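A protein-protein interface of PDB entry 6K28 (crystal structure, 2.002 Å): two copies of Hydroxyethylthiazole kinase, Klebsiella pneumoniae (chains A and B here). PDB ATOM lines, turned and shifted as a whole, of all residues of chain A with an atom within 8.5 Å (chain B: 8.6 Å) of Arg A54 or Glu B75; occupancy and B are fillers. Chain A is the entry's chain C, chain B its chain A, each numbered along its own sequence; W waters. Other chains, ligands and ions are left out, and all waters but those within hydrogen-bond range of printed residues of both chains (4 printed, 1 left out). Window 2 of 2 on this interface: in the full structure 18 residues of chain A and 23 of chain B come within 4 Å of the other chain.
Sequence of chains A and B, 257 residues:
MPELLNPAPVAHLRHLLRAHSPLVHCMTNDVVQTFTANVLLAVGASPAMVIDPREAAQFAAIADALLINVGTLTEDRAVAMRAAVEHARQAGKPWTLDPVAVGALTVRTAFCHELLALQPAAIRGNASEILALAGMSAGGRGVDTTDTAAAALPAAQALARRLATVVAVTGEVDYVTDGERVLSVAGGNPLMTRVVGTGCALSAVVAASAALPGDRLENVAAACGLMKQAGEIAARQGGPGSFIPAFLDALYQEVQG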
ATOM      1  N   HIS A  25     -43.536  17.726  -2.976  1.00  0.00           N
ATOM      2  CA  HIS A  25     -42.084  17.629  -3.059  1.00  0.00           C
ATOM      3  C   HIS A  25     -41.726  17.004  -4.412  1.00  0.00           C
ATOM      4  O   HIS A  25     -42.026  15.837  -4.652  1.00  0.00           O
ATOM      5  CB  HIS A  25     -41.567  16.784  -1.902  1.00  0.00           C
ATOM      6  CG  HIS A  25     -40.081  16.630  -1.857  1.00  0.00           C
ATOM      7  ND1 HIS A  25     -39.453  15.911  -0.863  1.00  0.00           N
ATOM      8  CD2 HIS A  25     -39.102  17.080  -2.673  1.00  0.00           C
ATOM      9  CE1 HIS A  25     -38.150  15.942  -1.065  1.00  0.00           C
ATOM     10  NE2 HIS A  25     -37.912  16.634  -2.163  1.00  0.00           N
ATOM     11  N   MET A  27     -38.985  15.730  -7.004  1.00  0.00           N
ATOM     12  CA  MET A  27     -37.653  15.320  -7.415  1.00  0.00           C
ATOM     13  C   MET A  27     -37.809  14.824  -8.857  1.00  0.00           C
ATOM     14  O   MET A  27     -38.146  13.661  -9.110  1.00  0.00           O
ATOM     15  CB  MET A  27     -37.077  14.263  -6.459  1.00  0.00           C
ATOM     16  CG  MET A  27     -37.164  14.683  -4.961  1.00  0.00           C
ATOM     17  SD  MET A  27     -36.279  13.692  -3.717  1.00  0.00           S
ATOM     18  CE  MET A  27     -34.597  14.011  -4.112  1.00  0.00           C
ATOM     19  N   VAL A  50     -36.613  19.989  -3.775  1.00  0.00           N
ATOM     20  CA  VAL A  50     -35.586  19.869  -2.757  1.00  0.00           C
ATOM     21  C   VAL A  50     -34.759  18.654  -3.041  1.00  0.00           C
ATOM     22  O   VAL A  50     -35.301  17.557  -3.092  1.00  0.00           O
ATOM     23  CB  VAL A  50     -36.193  19.749  -1.364  1.00  0.00           C
ATOM     24  CG1 VAL A  50     -35.084  19.636  -0.333  1.00  0.00           C
ATOM     25  CG2 VAL A  50     -37.101  20.962  -1.068  1.00  0.00           C
ATOM     26  N   ILE A  51     -33.445  18.815  -3.158  1.00  0.00           N
ATOM     27  CA  ILE A  51     -32.659  17.730  -3.745  1.00  0.00           C
ATOM     28  C   ILE A  51     -31.445  17.321  -2.942  1.00  0.00           C
ATOM     29  O   ILE A  51     -30.909  16.257  -3.194  1.00  0.00           O
ATOM     30  CB  ILE A  51     -32.204  18.082  -5.181  1.00  0.00           C
ATOM     31  CG1 ILE A  51     -31.449  19.401  -5.224  1.00  0.00           C
ATOM     32  CG2 ILE A  51     -33.438  18.181  -6.113  1.00  0.00           C
ATOM     33  CD1 ILE A  51     -30.789  19.672  -6.598  1.00  0.00           C
ATOM     34  N   ASP A  52     -30.991  18.152  -2.011  1.00  0.00           N
ATOM     35  CA  ASP A  52     -29.949  17.717  -1.095  1.00  0.00           C
ATOM     36  C   ASP A  52     -30.484  16.516  -0.279  1.00  0.00           C
ATOM     37  O   ASP A  52     -31.644  16.534   0.105  1.00  0.00           O
ATOM     38  CB  ASP A  52     -29.526  18.852  -0.167  1.00  0.00           C
ATOM     39  CG  ASP A  52     -28.627  18.367   0.962  1.00  0.00           C
ATOM     40  OD1 ASP A  52     -29.153  17.969   2.024  1.00  0.00           O
ATOM     41  OD2 ASP A  52     -27.392  18.387   0.783  1.00  0.00           O
ATOM     42  N   PRO A  53     -29.650  15.476  -0.026  1.00  0.00           N
ATOM     43  CA  PRO A  53     -30.150  14.294   0.707  1.00  0.00           C
ATOM     44  C   PRO A  53     -30.780  14.608   2.070  1.00  0.00           C
ATOM     45  O   PRO A  53     -31.874  14.124   2.402  1.00  0.00           O
ATOM     46  CB  PRO A  53     -28.888  13.435   0.918  1.00  0.00           C
ATOM     47  CG  PRO A  53     -27.933  13.874  -0.100  1.00  0.00           C
ATOM     48  CD  PRO A  53     -28.227  15.330  -0.386  1.00  0.00           C
ATOM     49  N   ARG A  54     -30.088  15.416   2.848  1.00  0.00           N
ATOM     50  CA  ARG A  54     -30.575  15.752   4.178  1.00  0.00           C
ATOM     51  C   ARG A  54     -31.839  16.626   4.104  1.00  0.00           C
ATOM     52  O   ARG A  54     -32.831  16.355   4.797  1.00  0.00           O
ATOM     53  CB  ARG A  54     -29.482  16.449   4.975  1.00  0.00           C
ATOM     54  CG  ARG A  54     -28.317  15.542   5.366  1.00  0.00           C
ATOM     55  CD  ARG A  54     -27.281  16.292   6.192  1.00  0.00           C
ATOM     56  NE  ARG A  54     -26.433  17.154   5.374  1.00  0.00           N
ATOM     57  CZ  ARG A  54     -25.642  18.101   5.871  1.00  0.00           C
ATOM     58  NH1 ARG A  54     -25.605  18.327   7.185  1.00  0.00           N
ATOM     59  NH2 ARG A  54     -24.889  18.830   5.053  1.00  0.00           N
ATOM     60  N   GLU A  55     -31.819  17.657   3.244  1.00  0.00           N
ATOM     61  CA  GLU A  55     -32.998  18.511   3.069  1.00  0.00           C
ATOM     62  C   GLU A  55     -34.170  17.700   2.536  1.00  0.00           C
ATOM     63  O   GLU A  55     -35.309  17.930   2.920  1.00  0.00           O
ATOM     64  CB  GLU A  55     -32.734  19.694   2.105  1.00  0.00           C
ATOM     65  CG  GLU A  55     -31.741  20.687   2.617  1.00  0.00           C
ATOM     66  CD  GLU A  55     -31.743  21.966   1.802  1.00  0.00           C
ATOM     67  OE1 GLU A  55     -32.135  21.936   0.607  1.00  0.00           O
ATOM     68  OE2 GLU A  55     -31.343  22.999   2.351  1.00  0.00           O
ATOM     69  N   ALA A  56     -33.918  16.787   1.605  1.00  0.00           N
ATOM     70  CA  ALA A  56     -35.017  16.050   0.997  1.00  0.00           C
ATOM     71  C   ALA A  56     -35.645  15.108   1.999  1.00  0.00           C
ATOM     72  O   ALA A  56     -36.859  14.876   1.955  1.00  0.00           O
ATOM     73  CB  ALA A  56     -34.555  15.267  -0.232  1.00  0.00           C
ATOM     74  N   ALA A  57     -34.809  14.512   2.856  1.00  0.00           N
ATOM     75  CA  ALA A  57     -35.327  13.691   3.950  1.00  0.00           C
ATOM     76  C   ALA A  57     -36.197  14.540   4.893  1.00  0.00           C
ATOM     77  O   ALA A  57     -37.306  14.144   5.270  1.00  0.00           O
ATOM     78  CB  ALA A  57     -34.191  13.043   4.715  1.00  0.00           C
ATOM     79  N   GLN A  58     -35.684  15.699   5.277  1.00  0.00           N
ATOM     80  CA  GLN A  58     -36.465  16.592   6.119  1.00  0.00           C
ATOM     81  C   GLN A  58     -37.783  16.947   5.449  1.00  0.00           C
ATOM     82  O   GLN A  58     -38.863  16.861   6.045  1.00  0.00           O
ATOM     83  CB  GLN A  58     -35.670  17.869   6.418  1.00  0.00           C
ATOM     84  CG  GLN A  58     -36.448  18.895   7.231  1.00  0.00           C
ATOM     85  CD  GLN A  58     -35.662  20.148   7.493  1.00  0.00           C
ATOM     86  OE1 GLN A  58     -34.595  20.364   6.907  1.00  0.00           O
ATOM     87  NE2 GLN A  58     -36.189  20.999   8.380  1.00  0.00           N
ATOM     88  N   PHE A  59     -37.704  17.358   4.191  1.00  0.00           N
ATOM     89  CA  PHE A  59     -38.863  17.964   3.565  1.00  0.00           C
ATOM     90  C   PHE A  59     -39.900  16.942   3.167  1.00  0.00           C
ATOM     91  O   PHE A  59     -41.082  17.242   3.149  1.00  0.00           O
ATOM     92  CB  PHE A  59     -38.445  18.789   2.341  1.00  0.00           C
ATOM     93  CG  PHE A  59     -39.563  19.574   1.771  1.00  0.00           C
ATOM     94  CD1 PHE A  59     -40.160  20.580   2.518  1.00  0.00           C
ATOM     95  CD2 PHE A  59     -40.063  19.282   0.522  1.00  0.00           C
ATOM     96  CE1 PHE A  59     -41.227  21.295   2.001  1.00  0.00           C
ATOM     97  CE2 PHE A  59     -41.125  19.990   0.003  1.00  0.00           C
ATOM     98  CZ  PHE A  59     -41.712  20.992   0.748  1.00  0.00           C
ATOM     99  N   ALA A  60     -39.456  15.743   2.804  1.00  0.00           N
ATOM    100  CA  ALA A  60     -40.385  14.681   2.400  1.00  0.00           C
ATOM    101  C   ALA A  60     -41.356  14.302   3.527  1.00  0.00           C
ATOM    102  O   ALA A  60     -42.462  13.826   3.275  1.00  0.00           O
ATOM    103  CB  ALA A  60     -39.592  13.436   1.917  1.00  0.00           C
ATOM    104  N   ALA A  61     -40.936  14.540   4.766  1.00  0.00           N
ATOM    105  CA  ALA A  61     -41.769  14.297   5.936  1.00  0.00           C
ATOM    106  C   ALA A  61     -42.868  15.346   6.058  1.00  0.00           C
ATOM    107  O   ALA A  61     -43.960  15.081   6.579  1.00  0.00           O
ATOM    108  CB  ALA A  61     -40.912  14.291   7.180  1.00  0.00           C
ATOM    109  N   ASP A  76     -25.823  10.622  -7.396  1.00  0.00           N
ATOM    110  CA  ASP A  76     -26.047  11.536  -6.264  1.00  0.00           C
ATOM    111  C   ASP A  76     -27.519  11.796  -6.036  1.00  0.00           C
ATOM    112  O   ASP A  76     -27.979  11.868  -4.887  1.00  0.00           O
ATOM    113  CB  ASP A  76     -25.339  12.880  -6.478  1.00  0.00           C
ATOM    114  CG  ASP A  76     -23.860  12.811  -6.193  1.00  0.00           C
ATOM    115  OD1 ASP A  76     -23.401  11.735  -5.736  1.00  0.00           O
ATOM    116  OD2 ASP A  76     -23.163  13.835  -6.410  1.00  0.00           O
ATOM    117  N   VAL A  79     -29.423   8.766  -4.606  1.00  0.00           N
ATOM    118  CA  VAL A  79     -29.259   8.743  -3.144  1.00  0.00           C
ATOM    119  C   VAL A  79     -30.300   9.627  -2.433  1.00  0.00           C
ATOM    120  O   VAL A  79     -30.980   9.190  -1.482  1.00  0.00           O
ATOM    121  CB  VAL A  79     -27.863   9.191  -2.725  1.00  0.00           C
ATOM    122  CG1 VAL A  79     -27.772   9.398  -1.198  1.00  0.00           C
ATOM    123  CG2 VAL A  79     -26.844   8.162  -3.169  1.00  0.00           C
ATOM    124  N   ALA A  80     -30.436  10.863  -2.906  1.00  0.00           N
ATOM    125  CA  ALA A  80     -31.370  11.800  -2.284  1.00  0.00           C
ATOM    126  C   ALA A  80     -32.795  11.288  -2.459  1.00  0.00           C
ATOM    127  O   ALA A  80     -33.618  11.360  -1.532  1.00  0.00           O
ATOM    128  CB  ALA A  80     -31.206  13.202  -2.876  1.00  0.00           C
ATOM    129  N   ALA A  83     -33.472   8.594   0.118  1.00  0.00           N
ATOM    130  CA  ALA A  83     -33.707   9.233   1.421  1.00  0.00           C
ATOM    131  C   ALA A  83     -35.113   9.867   1.540  1.00  0.00           C
ATOM    132  O   ALA A  83     -35.809   9.731   2.580  1.00  0.00           O
ATOM    133  CB  ALA A  83     -32.659  10.263   1.673  1.00  0.00           C
ATOM    134  N   ALA A  84     -35.534  10.544   0.467  1.00  0.00           N
ATOM    135  CA  ALA A  84     -36.858  11.158   0.422  1.00  0.00           C
ATOM    136  C   ALA A  84     -37.943  10.108   0.539  1.00  0.00           C
ATOM    137  O   ALA A  84     -38.855  10.224   1.374  1.00  0.00           O
ATOM    138  CB  ALA A  84     -37.046  11.954  -0.860  1.00  0.00           C
ATOM    139  N   HIS A  87     -38.224   8.615   4.068  1.00  0.00           N
ATOM    140  CA  HIS A  87     -38.820   9.506   5.058  1.00  0.00           C
ATOM    141  C   HIS A  87     -40.270   9.863   4.776  1.00  0.00           C
ATOM    142  O   HIS A  87     -41.024  10.097   5.696  1.00  0.00           O
ATOM    143  CB  HIS A  87     -37.969  10.758   5.187  1.00  0.00           C
ATOM    144  CG  HIS A  87     -36.679  10.504   5.883  1.00  0.00           C
ATOM    145  ND1 HIS A  87     -35.658   9.785   5.302  1.00  0.00           N
ATOM    146  CD2 HIS A  87     -36.254  10.835   7.125  1.00  0.00           C
ATOM    147  CE1 HIS A  87     -34.652   9.692   6.153  1.00  0.00           C
ATOM    148  NE2 HIS A  87     -34.987  10.326   7.264  1.00  0.00           N
ATOM    149  N   PRO B  53     -16.703  24.878  -9.303  1.00  0.00           N
ATOM    150  CA  PRO B  53     -16.054  25.726  -8.281  1.00  0.00           C
ATOM    151  C   PRO B  53     -14.848  26.533  -8.800  1.00  0.00           C
ATOM    152  O   PRO B  53     -14.638  27.710  -8.437  1.00  0.00           O
ATOM    153  CB  PRO B  53     -15.646  24.711  -7.196  1.00  0.00           C
ATOM    154  CG  PRO B  53     -15.681  23.383  -7.852  1.00  0.00           C
ATOM    155  CD  PRO B  53     -16.761  23.464  -8.892  1.00  0.00           C
ATOM    156  N   THR B  72     -32.328  25.287  -4.658  1.00  0.00           N
ATOM    157  CA  THR B  72     -32.117  23.855  -4.847  1.00  0.00           C
ATOM    158  C   THR B  72     -30.677  23.514  -4.471  1.00  0.00           C
ATOM    159  O   THR B  72     -29.952  22.886  -5.219  1.00  0.00           O
ATOM    160  CB  THR B  72     -32.426  23.383  -6.313  1.00  0.00           C
ATOM    161  OG1 THR B  72     -31.746  24.201  -7.271  1.00  0.00           O
ATOM    162  CG2 THR B  72     -33.953  23.423  -6.572  1.00  0.00           C
ATOM    163  N   LEU B  73     -30.290  23.958  -3.286  1.00  0.00           N
ATOM    164  CA  LEU B  73     -28.948  23.743  -2.772  1.00  0.00           C
ATOM    165  C   LEU B  73     -28.518  22.285  -2.724  1.00  0.00           C
ATOM    166  O   LEU B  73     -29.258  21.431  -2.249  1.00  0.00           O
ATOM    167  CB  LEU B  73     -28.835  24.299  -1.350  1.00  0.00           C
ATOM    168  CG  LEU B  73     -27.411  24.443  -0.792  1.00  0.00           C
ATOM    169  CD1 LEU B  73     -26.602  25.376  -1.640  1.00  0.00           C
ATOM    170  CD2 LEU B  73     -27.472  24.966   0.643  1.00  0.00           C
ATOM    171  N   THR B  74     -27.293  22.040  -3.152  1.00  0.00           N
ATOM    172  CA  THR B  74     -26.643  20.749  -2.942  1.00  0.00           C
ATOM    173  C   THR B  74     -25.261  20.965  -2.380  1.00  0.00           C
ATOM    174  O   THR B  74     -24.762  22.078  -2.359  1.00  0.00           O
ATOM    175  CB  THR B  74     -26.507  19.923  -4.232  1.00  0.00           C
ATOM    176  OG1 THR B  74     -25.827  20.700  -5.224  1.00  0.00           O
ATOM    177  CG2 THR B  74     -27.861  19.465  -4.744  1.00  0.00           C
ATOM    178  N   GLU B  75     -24.627  19.896  -1.919  1.00  0.00           N
ATOM    179  CA  GLU B  75     -23.312  20.012  -1.291  1.00  0.00           C
ATOM    180  C   GLU B  75     -22.234  20.566  -2.221  1.00  0.00           C
ATOM    181  O   GLU B  75     -21.522  21.498  -1.862  1.00  0.00           O
ATOM    182  CB  GLU B  75     -22.868  18.643  -0.747  1.00  0.00           C
ATOM    183  CG  GLU B  75     -23.685  18.202   0.417  1.00  0.00           C
ATOM    184  CD  GLU B  75     -22.981  17.168   1.290  1.00  0.00           C
ATOM    185  OE1 GLU B  75     -22.633  17.507   2.449  1.00  0.00           O
ATOM    186  OE2 GLU B  75     -22.786  16.022   0.817  1.00  0.00           O
ATOM    187  N   ASP B  76     -22.119  20.000  -3.418  1.00  0.00           N
ATOM    188  CA  ASP B  76     -21.156  20.462  -4.404  1.00  0.00           C
ATOM    189  C   ASP B  76     -21.379  21.942  -4.723  1.00  0.00           C
ATOM    190  O   ASP B  76     -20.441  22.763  -4.750  1.00  0.00           O
ATOM    191  CB  ASP B  76     -21.255  19.660  -5.713  1.00  0.00           C
ATOM    192  CG  ASP B  76     -20.728  18.213  -5.591  1.00  0.00           C
ATOM    193  OD1 ASP B  76     -20.016  17.901  -4.612  1.00  0.00           O
ATOM    194  OD2 ASP B  76     -21.034  17.392  -6.500  1.00  0.00           O
ATOM    195  N   ARG B  77     -22.635  22.276  -5.001  1.00  0.00           N
ATOM    196  CA  ARG B  77     -22.953  23.658  -5.373  1.00  0.00           C
ATOM    197  C   ARG B  77     -22.609  24.638  -4.247  1.00  0.00           C
ATOM    198  O   ARG B  77     -22.160  25.737  -4.530  1.00  0.00           O
ATOM    199  CB  ARG B  77     -24.424  23.803  -5.759  1.00  0.00           C
ATOM    200  CG  ARG B  77     -24.716  25.111  -6.535  1.00  0.00           C
ATOM    201  CD  ARG B  77     -23.996  25.178  -7.892  1.00  0.00           C
ATOM    202  NE  ARG B  77     -24.093  23.900  -8.590  1.00  0.00           N
ATOM    203  CZ  ARG B  77     -25.109  23.513  -9.353  1.00  0.00           C
ATOM    204  NH1 ARG B  77     -26.142  24.310  -9.582  1.00  0.00           N
ATOM    205  NH2 ARG B  77     -25.080  22.303  -9.890  1.00  0.00           N
ATOM    206  N   ALA B  78     -22.848  24.263  -2.995  1.00  0.00           N
ATOM    207  CA  ALA B  78     -22.497  25.126  -1.862  1.00  0.00           C
ATOM    208  C   ALA B  78     -21.016  25.469  -1.838  1.00  0.00           C
ATOM    209  O   ALA B  78     -20.617  26.601  -1.524  1.00  0.00           O
ATOM    210  CB  ALA B  78     -22.898  24.460  -0.543  1.00  0.00           C
ATOM    211  N   VAL B  79     -20.181  24.496  -2.190  1.00  0.00           N
ATOM    212  CA  VAL B  79     -18.740  24.736  -2.241  1.00  0.00           C
ATOM    213  C   VAL B  79     -18.398  25.726  -3.322  1.00  0.00           C
ATOM    214  O   VAL B  79     -17.568  26.647  -3.133  1.00  0.00           O
ATOM    215  CB  VAL B  79     -17.968  23.405  -2.488  1.00  0.00           C
ATOM    216  CG1 VAL B  79     -16.510  23.682  -2.813  1.00  0.00           C
ATOM    217  CG2 VAL B  79     -18.114  22.531  -1.236  1.00  0.00           C
ATOM    218  N   ALA B  80     -19.044  25.527  -4.472  1.00  0.00           N
ATOM    219  CA  ALA B  80     -18.832  26.424  -5.583  1.00  0.00           C
ATOM    220  C   ALA B  80     -19.324  27.832  -5.270  1.00  0.00           C
ATOM    221  O   ALA B  80     -18.641  28.816  -5.568  1.00  0.00           O
ATOM    222  CB  ALA B  80     -19.508  25.892  -6.827  1.00  0.00           C
ATOM    223  N   MET B  81     -20.473  27.919  -4.607  1.00  0.00           N
ATOM    224  CA  MET B  81     -21.046  29.215  -4.258  1.00  0.00           C
ATOM    225  C   MET B  81     -20.114  29.963  -3.271  1.00  0.00           C
ATOM    226  O   MET B  81     -19.850  31.150  -3.413  1.00  0.00           O
ATOM    227  CB  MET B  81     -22.437  29.010  -3.647  1.00  0.00           C
ATOM    228  CG  MET B  81     -23.580  28.621  -4.648  1.00  0.00           C
ATOM    229  SD  MET B  81     -25.124  28.108  -3.841  1.00  0.00           S
ATOM    230  CE  MET B  81     -26.198  28.164  -5.276  1.00  0.00           C
ATOM    231  N   ARG B  82     -19.651  29.268  -2.232  1.00  0.00           N
ATOM    232  CA  ARG B  82     -18.741  29.901  -1.270  1.00  0.00           C
ATOM    233  C   ARG B  82     -17.497  30.431  -1.979  1.00  0.00           C
ATOM    234  O   ARG B  82     -17.079  31.587  -1.737  1.00  0.00           O
ATOM    235  CB  ARG B  82     -18.377  28.907  -0.170  1.00  0.00           C
ATOM    236  CG  ARG B  82     -17.208  29.327   0.737  1.00  0.00           C
ATOM    237  CD  ARG B  82     -17.683  29.847   2.044  1.00  0.00           C
ATOM    238  NE  ARG B  82     -16.607  30.506   2.799  1.00  0.00           N
ATOM    239  CZ  ARG B  82     -16.731  30.925   4.052  1.00  0.00           C
ATOM    240  NH1 ARG B  82     -17.876  30.750   4.697  1.00  0.00           N
ATOM    241  NH2 ARG B  82     -15.713  31.512   4.659  1.00  0.00           N
ATOM    242  N   LEU B 105     -35.547  24.844   5.984  1.00  0.00           N
ATOM    243  CA  LEU B 105     -34.703  23.703   5.674  1.00  0.00           C
ATOM    244  C   LEU B 105     -33.331  23.935   6.281  1.00  0.00           C
ATOM    245  O   LEU B 105     -32.680  24.924   6.045  1.00  0.00           O
ATOM    246  CB  LEU B 105     -34.607  23.483   4.156  1.00  0.00           C
ATOM    247  CG  LEU B 105     -35.884  23.125   3.401  1.00  0.00           C
ATOM    248  CD1 LEU B 105     -35.681  23.271   1.882  1.00  0.00           C
ATOM    249  CD2 LEU B 105     -36.366  21.711   3.722  1.00  0.00           C
ATOM    250  N   THR B 106     -32.865  22.960   7.029  1.00  0.00           N
ATOM    251  CA  THR B 106     -31.705  23.119   7.866  1.00  0.00           C
ATOM    252  C   THR B 106     -30.395  23.393   7.140  1.00  0.00           C
ATOM    253  O   THR B 106     -29.666  24.352   7.472  1.00  0.00           O
ATOM    254  CB  THR B 106     -31.598  21.863   8.725  1.00  0.00           C
ATOM    255  OG1 THR B 106     -32.863  21.672   9.380  1.00  0.00           O
ATOM    256  CG2 THR B 106     -30.550  22.001   9.717  1.00  0.00           C
ATOM    257  N   VAL B 107     -30.081  22.589   6.123  1.00  0.00           N
ATOM    258  CA  VAL B 107     -28.773  22.715   5.473  1.00  0.00           C
ATOM    259  C   VAL B 107     -28.552  24.108   4.907  1.00  0.00           C
ATOM    260  O   VAL B 107     -27.504  24.731   5.118  1.00  0.00           O
ATOM    261  CB  VAL B 107     -28.594  21.691   4.331  1.00  0.00           C
ATOM    262  CG1 VAL B 107     -27.279  21.950   3.561  1.00  0.00           C
ATOM    263  CG2 VAL B 107     -28.650  20.267   4.879  1.00  0.00           C
ATOM    264  N   ARG B 108     -29.529  24.598   4.156  1.00  0.00           N
ATOM    265  CA  ARG B 108     -29.352  25.904   3.527  1.00  0.00           C
ATOM    266  C   ARG B 108     -29.380  27.038   4.556  1.00  0.00           C
ATOM    267  O   ARG B 108     -28.698  28.065   4.376  1.00  0.00           O
ATOM    268  CB  ARG B 108     -30.424  26.143   2.465  1.00  0.00           C
ATOM    269  CG  ARG B 108     -31.824  26.050   2.976  1.00  0.00           C
ATOM    270  CD  ARG B 108     -32.831  26.131   1.818  1.00  0.00           C
ATOM    271  NE  ARG B 108     -32.789  24.949   0.951  1.00  0.00           N
ATOM    272  CZ  ARG B 108     -33.481  24.839  -0.178  1.00  0.00           C
ATOM    273  NH1 ARG B 108     -34.262  25.851  -0.588  1.00  0.00           N
ATOM    274  NH2 ARG B 108     -33.391  23.736  -0.902  1.00  0.00           N
ATOM    275  N   ALA B 110     -28.103  26.896   7.688  1.00  0.00           N
ATOM    276  CA  ALA B 110     -26.736  26.990   8.203  1.00  0.00           C
ATOM    277  C   ALA B 110     -25.781  27.609   7.193  1.00  0.00           C
ATOM    278  O   ALA B 110     -24.903  28.449   7.526  1.00  0.00           O
ATOM    279  CB  ALA B 110     -26.222  25.580   8.611  1.00  0.00           C
ATOM    280  N   PHE B 111     -25.931  27.175   5.939  1.00  0.00           N
ATOM    281  CA  PHE B 111     -25.054  27.682   4.886  1.00  0.00           C
ATOM    282  C   PHE B 111     -25.146  29.196   4.725  1.00  0.00           C
ATOM    283  O   PHE B 111     -24.138  29.907   4.599  1.00  0.00           O
ATOM    284  CB  PHE B 111     -25.386  26.998   3.551  1.00  0.00           C
ATOM    285  CG  PHE B 111     -24.523  27.464   2.399  1.00  0.00           C
ATOM    286  CD1 PHE B 111     -23.157  27.250   2.406  1.00  0.00           C
ATOM    287  CD2 PHE B 111     -25.088  28.088   1.303  1.00  0.00           C
ATOM    288  CE1 PHE B 111     -22.378  27.658   1.347  1.00  0.00           C
ATOM    289  CE2 PHE B 111     -24.324  28.496   0.244  1.00  0.00           C
ATOM    290  CZ  PHE B 111     -22.963  28.272   0.248  1.00  0.00           C
HETATM  291  O   HOH W   1     -26.375  21.192   0.437  1.00  0.00           O
HETATM  292  O   HOH W   2     -25.355  18.976   2.682  1.00  0.00           O
HETATM  293  O   HOH W   3     -26.063  17.626  -1.762  1.00  0.00           O
HETATM  294  O   HOH W   4     -32.089  19.884   6.108  1.00  0.00           O
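4 positions are printed for both chains.
No residue of chain B comes within 4 Å of Pro A53. Arg A54 touches just these residues of chain B: Glu B75 and Val B107. Ala A60 touches none of the printed residues of chain B. Of chain A, only Asp A52 and Arg A54 come within 4 Å of Glu B75. Of the printed residues of chain A, Leu B105 touches Glu A55 (3.8 Å), Gln A58 (3.6 Å) and Phe A59 (3.8 Å). Of the printed residues of chain A, Arg B108 touches Glu A55 (2.7 Å). Ala B110 touches none of the printed residues of chain A. The nearest printed residue of chain A that does not touch Leu B105 is Val A50 (4.01 Å).
CD1 of Ile A51 touches O of Thr B72, 3.6 Å away. Ile A51 touches Thr B74 (CD1 to CG2, 3.5 Å). Asp A52 touches Leu B73. Asp A52 touches Glu B75. Asp A52 touches Val B107 (OD1 to CG2, 3.7 Å). Arg A54 touches Val B107 (CZ to CG2, 3.8 Å). OE2 of Glu A55 touches CB of Leu B105, 3.8 Å away. Glu A55 touches Val B107. OE1 of Gln A58 touches CA of Leu B105, at 3.6 Å. Phe A59 touches Leu B105 (CB to CD2, 3.8 Å).
The side-chain carboxylate (OE1) of Glu B75 is in salt-bridge range of the guanidinium group (NH2) of Arg A54, at 3.7 Å. The side-chain amide oxygen (OE1) of Gln A58 lies within hydrogen-bond range of the backbone NH (N) of Thr B106 (3.1 Å). The side-chain carboxylate of Glu A55 lies within salt-bridge range of the guanidinium group of Arg B108 (2.7 Å).
OD1 of Asp A52 lies within hydrogen-bond range of N of Arg A54 (2.8 Å). OD1 of Asp A52 sits at hydrogen-bond distance from N of Glu A55 (2.9 Å).
Water W2 lies within hydrogen-bond range of the guanidinium group (NH2) of Arg A54 (2.4 Å), the side-chain carboxylate (OD2) of Asp A52 (2.8 Å) and the side-chain carboxylate (OE1) of Glu B75 (3.1 Å). Water W4 lies within hydrogen-bond range of OE1 of Gln A58 (2.7 Å), N of Thr B106 (3.3 Å) and N of Val B107 (3.4 Å). Water W3 lies within hydrogen-bond range of the backbone NH (N) of Glu B75 (2.7 Å) and the side-chain carboxylate (OD2) of Asp A52 (3.0 Å). Water W1 lies within hydrogen-bond range of OD2 of Asp A52 (3.0 Å), N of Glu B75 (3.2 Å) and O of Thr B74 (3.3 Å).
Of the 18 printed residues of chain B, 8 touch a printed residue of chain A. Hydrophobic or aromatic side chains of chain A that line the printed part of chain B: Ile A51 and Phe A59. Among the printed residues, Asp or Glu carboxylates within 4 Å of a Lys or Arg side-chain nitrogen of the other chain: Arg A54 with Glu B75 (3.7 Å) and Glu A55 with Arg B108 (2.7 Å).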
